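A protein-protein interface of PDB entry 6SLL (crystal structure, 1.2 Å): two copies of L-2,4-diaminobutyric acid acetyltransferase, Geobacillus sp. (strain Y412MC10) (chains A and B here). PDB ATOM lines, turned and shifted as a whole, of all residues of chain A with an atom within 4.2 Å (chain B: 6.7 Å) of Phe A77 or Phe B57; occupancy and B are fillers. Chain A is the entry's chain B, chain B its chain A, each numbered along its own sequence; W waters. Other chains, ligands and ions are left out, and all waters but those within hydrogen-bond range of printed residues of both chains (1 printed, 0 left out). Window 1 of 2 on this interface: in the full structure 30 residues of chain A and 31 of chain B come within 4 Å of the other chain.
Water W1 bridges O of Tyr B56 and OG of Ser A79.
Phe B57 touches just these residues of chain A: Phe A77 (3.6 Å) and Pro A80 (3.8 Å).
Of the printed residues of chain A, Phe B77 touches Phe A57.
Of the printed residues of chain A, Pro B80 touches Phe A57.
Of the printed residues of chain B, Ser A79 touches Tyr B56 (3.7 Å).
Gly B54 touches none of the printed residues of chain A.
Cys B61 touches none of the printed residues of chain A.
Of the 19 printed residues of chain B, 5 touch a printed residue of chain A.
Printed residues of chain B that touch a printed residue of chain A: Leu B52, Tyr B56, Phe B57, Phe B77 and Pro B80.
Hydrophobic or aromatic side chains of chain B that line the printed part of chain A: Leu B52, Tyr B56, Phe B57, Phe B77 and Pro B80.
Hydrophobic or aromatic side chains of chain A that line the printed part of chain B: Phe A57, Phe A77, Pro A80 and Phe A87.
N of Ser A79 lies within hydrogen-bond range of O of Thr A85 (2.9 Å).
The backbone carbonyl oxygen (O) of Phe B57 is in hydrogen-bond range of the side-chain sulfur (SG) of Cys B61, at 3.4 Å.
O of Phe A57 is in hydrogen-bond range of OG1 of Thr A60.
The backbone carbonyl oxygen (O) of Phe A77 is in hydrogen-bond range of the backbone NH (N) of Phe A87 (2.8 Å).
The backbone carbonyl oxygen (O) of Phe B57 sits at hydrogen-bond distance from the side-chain hydroxyl (OG1) of Thr B60 (3.2 Å).
Phe A57 touches Phe B77, and with the chains exchanged Phe A77 touches Phe B57.
Phe A57 touches Pro B80, and with the chains exchanged Pro A80 touches Phe B57.
6 positions are printed for both chains.
Phe A57 touches Phe B77.
CE1 of Phe A57 touches CG of Pro B80, at 3.7 Å.
Tyr B56 touches Phe A77.
CE2 of Phe B57 touches CZ of Phe A77, 3.6 Å away.
Ser A79 touches Tyr B56.
O of Tyr B56 touches CD of Pro A80 (3.5 Å).
Pro A80 touches Phe B57.
Phe A87 touches Leu B52.
CD1 of Phe A87 touches OH of Tyr B56, 3.1 Å away.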
ATOM      1  N   PHE A  57      19.639  -9.424 -12.822  1.00  0.00           N
ATOM      2  CA  PHE A  57      20.458  -8.275 -13.155  1.00  0.00           C
ATOM      3  C   PHE A  57      20.397  -7.890 -14.620  1.00  0.00           C
ATOM      4  O   PHE A  57      21.152  -7.063 -15.105  1.00  0.00           O
ATOM      5  CB  PHE A  57      21.896  -8.410 -12.681  1.00  0.00           C
ATOM      6  CG  PHE A  57      22.031  -8.508 -11.218  1.00  0.00           C
ATOM      7  CD1 PHE A  57      22.080  -7.336 -10.432  1.00  0.00           C
ATOM      8  CD2 PHE A  57      22.075  -9.688 -10.560  1.00  0.00           C
ATOM      9  CE1 PHE A  57      22.218  -7.409  -9.073  1.00  0.00           C
ATOM     10  CE2 PHE A  57      22.174  -9.765  -9.178  1.00  0.00           C
ATOM     11  CZ  PHE A  57      22.257  -8.616  -8.433  1.00  0.00           C
ATOM     12  N   THR A  60      20.715  -4.443 -16.576  1.00  0.00           N
ATOM     13  CA  THR A  60      21.989  -3.750 -16.612  1.00  0.00           C
ATOM     14  C   THR A  60      23.105  -4.664 -17.134  1.00  0.00           C
ATOM     15  O   THR A  60      24.264  -4.417 -16.751  1.00  0.00           O
ATOM     16  CB  THR A  60      22.330  -3.159 -15.237  1.00  0.00           C
ATOM     17  OG1 THR A  60      22.392  -4.196 -14.252  1.00  0.00           O
ATOM     18  CG2 THR A  60      21.359  -2.119 -14.806  1.00  0.00           C
ATOM     19  N   ALA A  76      26.918  -5.954 -15.237  1.00  0.00           N
ATOM     20  CA  ALA A  76      27.013  -4.758 -14.426  1.00  0.00           C
ATOM     21  C   ALA A  76      25.834  -4.742 -13.526  1.00  0.00           C
ATOM     22  O   ALA A  76      24.808  -5.402 -13.707  1.00  0.00           O
ATOM     23  CB  ALA A  76      27.013  -3.509 -15.310  1.00  0.00           C
ATOM     24  N   PHE A  77      25.894  -3.860 -12.488  1.00  0.00           N
ATOM     25  CA  PHE A  77      24.793  -3.639 -11.537  1.00  0.00           C
ATOM     26  C   PHE A  77      24.909  -2.271 -10.956  1.00  0.00           C
ATOM     27  O   PHE A  77      26.038  -1.728 -10.831  1.00  0.00           O
ATOM     28  CB  PHE A  77      24.704  -4.729 -10.453  1.00  0.00           C
ATOM     29  CG  PHE A  77      25.972  -4.867  -9.653  1.00  0.00           C
ATOM     30  CD1 PHE A  77      26.303  -4.009  -8.611  1.00  0.00           C
ATOM     31  CD2 PHE A  77      26.887  -5.845  -9.957  1.00  0.00           C
ATOM     32  CE1 PHE A  77      27.512  -4.122  -7.922  1.00  0.00           C
ATOM     33  CE2 PHE A  77      28.072  -5.971  -9.232  1.00  0.00           C
ATOM     34  CZ  PHE A  77      28.400  -5.128  -8.224  1.00  0.00           C
ATOM     35  N   ARG A  78      23.796  -1.644 -10.611  1.00  0.00           N
ATOM     36  CA  ARG A  78      23.859  -0.400  -9.872  1.00  0.00           C
ATOM     37  C   ARG A  78      24.204  -0.678  -8.418  1.00  0.00           C
ATOM     38  O   ARG A  78      23.680  -1.597  -7.801  1.00  0.00           O
ATOM     39  CB  ARG A  78      22.554   0.384  -9.990  1.00  0.00           C
ATOM     40  CG  ARG A  78      22.256   0.704 -11.400  1.00  0.00           C
ATOM     41  CD  ARG A  78      21.435   1.644 -11.793  1.00  0.00           C
ATOM     42  NE  ARG A  78      21.603   3.023 -11.312  1.00  0.00           N
ATOM     43  CZ  ARG A  78      21.006   4.011 -11.880  1.00  0.00           C
ATOM     44  NH1 ARG A  78      20.222   3.835 -12.904  1.00  0.00           N
ATOM     45  NH2 ARG A  78      21.105   5.232 -11.335  1.00  0.00           N
ATOM     46  N   SER A  79      25.136   0.108  -7.850  1.00  0.00           N
ATOM     47  CA  SER A  79      25.533  -0.146  -6.455  1.00  0.00           C
ATOM     48  C   SER A  79      24.347   0.063  -5.524  1.00  0.00           C
ATOM     49  O   SER A  79      23.806   1.146  -5.517  1.00  0.00           O
ATOM     50  CB  SER A  79      26.685   0.828  -6.161  1.00  0.00           C
ATOM     51  OG  SER A  79      26.974   0.732  -4.766  1.00  0.00           O
ATOM     52  N   PRO A  80      24.055  -0.901  -4.682  1.00  0.00           N
ATOM     53  CA  PRO A  80      22.887  -0.695  -3.802  1.00  0.00           C
ATOM     54  C   PRO A  80      22.974   0.501  -2.896  1.00  0.00           C
ATOM     55  O   PRO A  80      21.963   1.273  -2.777  1.00  0.00           O
ATOM     56  CB  PRO A  80      22.841  -2.024  -3.018  1.00  0.00           C
ATOM     57  CG  PRO A  80      23.328  -3.032  -3.990  1.00  0.00           C
ATOM     58  CD  PRO A  80      24.444  -2.321  -4.734  1.00  0.00           C
ATOM     59  N   THR A  85      26.073   5.046  -9.086  1.00  0.00           N
ATOM     60  CA  THR A  85      27.223   4.319  -9.599  1.00  0.00           C
ATOM     61  C   THR A  85      26.798   2.999 -10.270  1.00  0.00           C
ATOM     62  O   THR A  85      26.129   2.214  -9.582  1.00  0.00           O
ATOM     63  CB  THR A  85      28.238   4.055  -8.497  1.00  0.00           C
ATOM     64  OG1 THR A  85      28.775   5.331  -8.077  1.00  0.00           O
ATOM     65  CG2 THR A  85      29.373   3.189  -8.979  1.00  0.00           C
ATOM     66  N   LEU A  86      27.205   2.797 -11.489  1.00  0.00           N
ATOM     67  CA  LEU A  86      27.095   1.482 -12.143  1.00  0.00           C
ATOM     68  C   LEU A  86      28.467   0.796 -12.027  1.00  0.00           C
ATOM     69  O   LEU A  86      29.468   1.315 -12.493  1.00  0.00           O
ATOM     70  CB  LEU A  86      26.735   1.658 -13.590  1.00  0.00           C
ATOM     71  CG  LEU A  86      26.519   0.364 -14.366  1.00  0.00           C
ATOM     72  CD1 LEU A  86      25.198  -0.284 -14.028  1.00  0.00           C
ATOM     73  CD2 LEU A  86      26.577   0.608 -15.867  1.00  0.00           C
ATOM     74  N   PHE A  87      28.465  -0.405 -11.405  1.00  0.00           N
ATOM     75  CA  PHE A  87      29.681  -1.219 -11.347  1.00  0.00           C
ATOM     76  C   PHE A  87      29.681  -2.173 -12.536  1.00  0.00           C
ATOM     77  O   PHE A  87      28.709  -2.944 -12.696  1.00  0.00           O
ATOM     78  CB  PHE A  87      29.730  -2.006 -10.025  1.00  0.00           C
ATOM     79  CG  PHE A  87      31.033  -2.774  -9.926  1.00  0.00           C
ATOM     80  CD1 PHE A  87      32.159  -2.165  -9.510  1.00  0.00           C
ATOM     81  CD2 PHE A  87      31.088  -4.089 -10.250  1.00  0.00           C
ATOM     82  CE1 PHE A  87      33.343  -2.837  -9.416  1.00  0.00           C
ATOM     83  CE2 PHE A  87      32.278  -4.792 -10.150  1.00  0.00           C
ATOM     84  CZ  PHE A  87      33.421  -4.132  -9.743  1.00  0.00           C
ATOM     85  N   PRO B  24      29.892  -8.810   6.150  1.00  0.00           N
ATOM     86  CA  PRO B  24      31.191  -8.974   5.536  1.00  0.00           C
ATOM     87  C   PRO B  24      31.746  -7.644   5.008  1.00  0.00           C
ATOM     88  O   PRO B  24      31.014  -6.660   4.881  1.00  0.00           O
ATOM     89  CB  PRO B  24      30.920  -9.932   4.377  1.00  0.00           C
ATOM     90  CG  PRO B  24      29.523  -9.612   3.954  1.00  0.00           C
ATOM     91  CD  PRO B  24      28.781  -9.270   5.300  1.00  0.00           C
ATOM     92  N   CYS B  49      34.318 -12.524  -6.773  1.00  0.00           N
ATOM     93  CA  CYS B  49      32.865 -12.430  -6.511  1.00  0.00           C
ATOM     94  C   CYS B  49      32.614 -12.174  -5.061  1.00  0.00           C
ATOM     95  O   CYS B  49      31.751 -11.361  -4.675  1.00  0.00           O
ATOM     96  CB  CYS B  49      32.228 -13.735  -6.973  1.00  0.00           C
ATOM     97  SG  CYS B  49      30.437 -13.801  -6.768  1.00  0.00           S
ATOM     98  N   MET B  51      34.593 -10.872  -2.831  1.00  0.00           N
ATOM     99  CA  MET B  51      35.001  -9.502  -2.524  1.00  0.00           C
ATOM    100  C   MET B  51      33.932  -8.493  -2.904  1.00  0.00           C
ATOM    101  O   MET B  51      33.609  -7.592  -2.136  1.00  0.00           O
ATOM    102  CB  MET B  51      36.301  -9.158  -3.250  1.00  0.00           C
ATOM    103  CG  MET B  51      37.467 -10.024  -2.797  1.00  0.00           C
ATOM    104  SD  MET B  51      38.925  -9.658  -3.828  1.00  0.00           S
ATOM    105  CE  MET B  51      39.965 -11.019  -3.326  1.00  0.00           C
ATOM    106  N   LEU B  52      33.296  -8.671  -4.064  1.00  0.00           N
ATOM    107  CA  LEU B  52      32.218  -7.773  -4.493  1.00  0.00           C
ATOM    108  C   LEU B  52      31.090  -7.902  -3.552  1.00  0.00           C
ATOM    109  O   LEU B  52      30.435  -6.871  -3.237  1.00  0.00           O
ATOM    110  CB  LEU B  52      31.651  -8.121  -5.850  1.00  0.00           C
ATOM    111  CG  LEU B  52      32.546  -7.914  -7.029  1.00  0.00           C
ATOM    112  CD1 LEU B  52      31.725  -8.217  -8.302  1.00  0.00           C
ATOM    113  CD2 LEU B  52      33.108  -6.491  -7.119  1.00  0.00           C
ATOM    114  N   LEU B  53      30.717  -9.063  -3.100  1.00  0.00           N
ATOM    115  CA  LEU B  53      29.626  -9.197  -2.149  1.00  0.00           C
ATOM    116  C   LEU B  53      29.917  -8.451  -0.899  1.00  0.00           C
ATOM    117  O   LEU B  53      29.068  -7.736  -0.341  1.00  0.00           O
ATOM    118  CB  LEU B  53      29.274 -10.650  -1.898  1.00  0.00           C
ATOM    119  CG  LEU B  53      28.625 -11.345  -3.072  1.00  0.00           C
ATOM    120  CD1 LEU B  53      28.709 -12.874  -2.909  1.00  0.00           C
ATOM    121  CD2 LEU B  53      27.149 -10.904  -3.207  1.00  0.00           C
ATOM    122  N   GLY B  54      31.142  -8.555  -0.374  1.00  0.00           N
ATOM    123  CA  GLY B  54      31.535  -7.817   0.807  1.00  0.00           C
ATOM    124  C   GLY B  54      31.639  -6.331   0.595  1.00  0.00           C
ATOM    125  O   GLY B  54      31.564  -5.611   1.592  1.00  0.00           O
ATOM    126  N   ASP B  55      31.856  -5.875  -0.604  1.00  0.00           N
ATOM    127  CA  ASP B  55      31.973  -4.471  -0.910  1.00  0.00           C
ATOM    128  C   ASP B  55      30.649  -3.839  -1.193  1.00  0.00           C
ATOM    129  O   ASP B  55      30.104  -3.061  -0.429  1.00  0.00           O
ATOM    130  CB  ASP B  55      32.959  -4.272  -2.018  1.00  0.00           C
ATOM    131  CG  ASP B  55      33.366  -2.885  -2.314  1.00  0.00           C
ATOM    132  OD1 ASP B  55      32.552  -2.007  -1.875  1.00  0.00           O
ATOM    133  OD2 ASP B  55      34.398  -2.727  -3.003  1.00  0.00           O
ATOM    134  N   TYR B  56      29.997  -4.229  -2.247  1.00  0.00           N
ATOM    135  CA  TYR B  56      28.778  -3.618  -2.758  1.00  0.00           C
ATOM    136  C   TYR B  56      27.498  -4.141  -2.112  1.00  0.00           C
ATOM    137  O   TYR B  56      26.502  -3.387  -2.101  1.00  0.00           O
ATOM    138  CB  TYR B  56      28.722  -3.741  -4.271  1.00  0.00           C
ATOM    139  CG  TYR B  56      29.819  -3.022  -4.992  1.00  0.00           C
ATOM    140  CD1 TYR B  56      29.684  -1.673  -5.276  1.00  0.00           C
ATOM    141  CD2 TYR B  56      30.994  -3.627  -5.355  1.00  0.00           C
ATOM    142  CE1 TYR B  56      30.705  -0.952  -5.865  1.00  0.00           C
ATOM    143  CE2 TYR B  56      32.017  -2.942  -5.934  1.00  0.00           C
ATOM    144  CZ  TYR B  56      31.863  -1.593  -6.192  1.00  0.00           C
ATOM    145  OH  TYR B  56      32.928  -0.886  -6.737  1.00  0.00           O
ATOM    146  N   PHE B  57      27.483  -5.398  -1.685  1.00  0.00           N
ATOM    147  CA  PHE B  57      26.249  -6.068  -1.198  1.00  0.00           C
ATOM    148  C   PHE B  57      26.247  -6.308   0.271  1.00  0.00           C
ATOM    149  O   PHE B  57      25.407  -7.048   0.764  1.00  0.00           O
ATOM    150  CB  PHE B  57      25.964  -7.340  -2.002  1.00  0.00           C
ATOM    151  CG  PHE B  57      25.682  -7.069  -3.456  1.00  0.00           C
ATOM    152  CD1 PHE B  57      24.413  -6.745  -3.875  1.00  0.00           C
ATOM    153  CD2 PHE B  57      26.690  -7.149  -4.407  1.00  0.00           C
ATOM    154  CE1 PHE B  57      24.160  -6.490  -5.234  1.00  0.00           C
ATOM    155  CE2 PHE B  57      26.433  -6.938  -5.745  1.00  0.00           C
ATOM    156  CZ  PHE B  57      25.118  -6.635  -6.135  1.00  0.00           C
ATOM    157  N   ASN B  58      27.193  -5.714   1.044  1.00  0.00           N
ATOM    158  CA  ASN B  58      27.394  -6.189   2.419  1.00  0.00           C
ATOM    159  C   ASN B  58      26.210  -5.957   3.316  1.00  0.00           C
ATOM    160  O   ASN B  58      26.006  -6.689   4.293  1.00  0.00           O
ATOM    161  CB  ASN B  58      28.688  -5.728   3.020  1.00  0.00           C
ATOM    162  CG  ASN B  58      28.774  -4.293   3.179  1.00  0.00           C
ATOM    163  OD1 ASN B  58      27.899  -3.636   3.807  1.00  0.00           O
ATOM    164  ND2 ASN B  58      29.897  -3.751   2.734  1.00  0.00           N
ATOM    165  N   ASP B  59      25.385  -4.970   2.976  1.00  0.00           N
ATOM    166  CA  ASP B  59      24.249  -4.686   3.805  1.00  0.00           C
ATOM    167  C   ASP B  59      23.223  -5.761   3.844  1.00  0.00           C
ATOM    168  O   ASP B  59      22.444  -5.836   4.797  1.00  0.00           O
ATOM    169  CB  ASP B  59      23.548  -3.374   3.305  1.00  0.00           C
ATOM    170  CG  ASP B  59      24.549  -2.226   3.225  1.00  0.00           C
ATOM    171  OD1 ASP B  59      24.752  -1.587   4.221  1.00  0.00           O
ATOM    172  OD2 ASP B  59      25.271  -2.146   2.174  1.00  0.00           O
ATOM    173  N   THR B  60      23.241  -6.678   2.864  1.00  0.00           N
ATOM    174  CA  THR B  60      22.342  -7.815   2.770  1.00  0.00           C
ATOM    175  C   THR B  60      23.074  -9.147   2.822  1.00  0.00           C
ATOM    176  O   THR B  60      22.525 -10.149   2.392  1.00  0.00           O
ATOM    177  CB  THR B  60      21.418  -7.706   1.544  1.00  0.00           C
ATOM    178  OG1 THR B  60      22.247  -7.558   0.366  1.00  0.00           O
ATOM    179  CG2 THR B  60      20.523  -6.556   1.596  1.00  0.00           C
ATOM    180  N   CYS B  61      24.272  -9.150   3.427  1.00  0.00           N
ATOM    181  CA  CYS B  61      25.007 -10.384   3.652  1.00  0.00           C
ATOM    182  C   CYS B  61      25.391 -10.558   5.114  1.00  0.00           C
ATOM    183  O   CYS B  61      25.189  -9.589   5.905  1.00  0.00           O
ATOM    184  CB  CYS B  61      26.281 -10.405   2.788  1.00  0.00           C
ATOM    185  SG  CYS B  61      26.017 -10.393   1.013  1.00  0.00           S
ATOM    186  N   MET B  62      26.058 -11.634   5.437  1.00  0.00           N
ATOM    187  CA  MET B  62      26.430 -11.857   6.819  1.00  0.00           C
ATOM    188  C   MET B  62      27.439 -12.919   6.924  1.00  0.00           C
ATOM    189  O   MET B  62      27.510 -13.847   6.147  1.00  0.00           O
ATOM    190  CB  MET B  62      25.308 -12.201   7.730  1.00  0.00           C
ATOM    191  CG  MET B  62      25.825 -12.141   9.158  1.00  0.00           C
ATOM    192  SD  MET B  62      24.934 -10.992   9.807  1.00  0.00           S
ATOM    193  CE  MET B  62      24.141 -12.288  10.499  1.00  0.00           C
ATOM    194  N   ALA B  76      23.074 -12.407  -0.094  1.00  0.00           N
ATOM    195  CA  ALA B  76      21.731 -12.076  -0.537  1.00  0.00           C
ATOM    196  C   ALA B  76      21.763 -10.669  -1.119  1.00  0.00           C
ATOM    197  O   ALA B  76      22.704  -9.911  -0.912  1.00  0.00           O
ATOM    198  CB  ALA B  76      20.710 -12.149   0.616  1.00  0.00           C
ATOM    199  N   PHE B  77      20.712 -10.353  -1.879  1.00  0.00           N
ATOM    200  CA  PHE B  77      20.519  -9.023  -2.433  1.00  0.00           C
ATOM    201  C   PHE B  77      19.101  -8.763  -2.656  1.00  0.00           C
ATOM    202  O   PHE B  77      18.311  -9.706  -2.884  1.00  0.00           O
ATOM    203  CB  PHE B  77      21.333  -8.824  -3.764  1.00  0.00           C
ATOM    204  CG  PHE B  77      21.025  -9.831  -4.822  1.00  0.00           C
ATOM    205  CD1 PHE B  77      19.926  -9.763  -5.637  1.00  0.00           C
ATOM    206  CD2 PHE B  77      21.832 -10.958  -4.983  1.00  0.00           C
ATOM    207  CE1 PHE B  77      19.627 -10.701  -6.586  1.00  0.00           C
ATOM    208  CE2 PHE B  77      21.512 -11.890  -5.958  1.00  0.00           C
ATOM    209  CZ  PHE B  77      20.423 -11.796  -6.742  1.00  0.00           C
ATOM    210  N   ARG B  78      18.668  -7.516  -2.597  1.00  0.00           N
ATOM    211  CA  ARG B  78      17.300  -7.195  -2.978  1.00  0.00           C
ATOM    212  C   ARG B  78      17.207  -7.142  -4.486  1.00  0.00           C
ATOM    213  O   ARG B  78      18.051  -6.591  -5.166  1.00  0.00           O
ATOM    214  CB  ARG B  78      16.856  -5.840  -2.343  1.00  0.00           C
ATOM    215  CG  ARG B  78      16.806  -5.967  -0.823  1.00  0.00           C
ATOM    216  CD  ARG B  78      16.382  -4.786  -0.019  1.00  0.00           C
ATOM    217  NE  ARG B  78      14.933  -4.559  -0.172  1.00  0.00           N
ATOM    218  CZ  ARG B  78      14.191  -3.854   0.646  1.00  0.00           C
ATOM    219  NH1 ARG B  78      14.658  -3.449   1.821  1.00  0.00           N
ATOM    220  NH2 ARG B  78      12.898  -3.717   0.388  1.00  0.00           N
ATOM    221  N   PRO B  80      16.809  -6.130  -8.057  1.00  0.00           N
ATOM    222  CA  PRO B  80      16.752  -4.763  -8.600  1.00  0.00           C
ATOM    223  C   PRO B  80      15.411  -4.400  -9.145  1.00  0.00           C
ATOM    224  O   PRO B  80      14.941  -3.262  -8.852  1.00  0.00           O
ATOM    225  CB  PRO B  80      17.860  -4.778  -9.656  1.00  0.00           C
ATOM    226  CG  PRO B  80      18.906  -5.716  -9.094  1.00  0.00           C
ATOM    227  CD  PRO B  80      18.048  -6.808  -8.447  1.00  0.00           C
ATOM    228  N   TRP B  89      21.219 -16.114  -2.013  1.00  0.00           N
ATOM    229  CA  TRP B  89      22.063 -16.811  -2.964  1.00  0.00           C
ATOM    230  C   TRP B  89      22.746 -18.025  -2.382  1.00  0.00           C
ATOM    231  O   TRP B  89      22.433 -19.153  -2.788  1.00  0.00           O
ATOM    232  CB  TRP B  89      23.029 -15.798  -3.565  1.00  0.00           C
ATOM    233  CG  TRP B  89      23.906 -16.285  -4.663  1.00  0.00           C
ATOM    234  CD1 TRP B  89      24.046 -17.506  -5.204  1.00  0.00           C
ATOM    235  CD2 TRP B  89      24.852 -15.486  -5.357  1.00  0.00           C
ATOM    236  NE1 TRP B  89      25.018 -17.486  -6.166  1.00  0.00           N
ATOM    237  CE2 TRP B  89      25.518 -16.252  -6.307  1.00  0.00           C
ATOM    238  CE3 TRP B  89      25.160 -14.082  -5.302  1.00  0.00           C
ATOM    239  CZ2 TRP B  89      26.487 -15.729  -7.140  1.00  0.00           C
ATOM    240  CZ3 TRP B  89      26.104 -13.586  -6.173  1.00  0.00           C
ATOM    241  CH2 TRP B  89      26.751 -14.419  -7.078  1.00  0.00           C
HETATM  242  O   HOH W   1      26.492  -0.631  -2.395  1.00  0.00           O
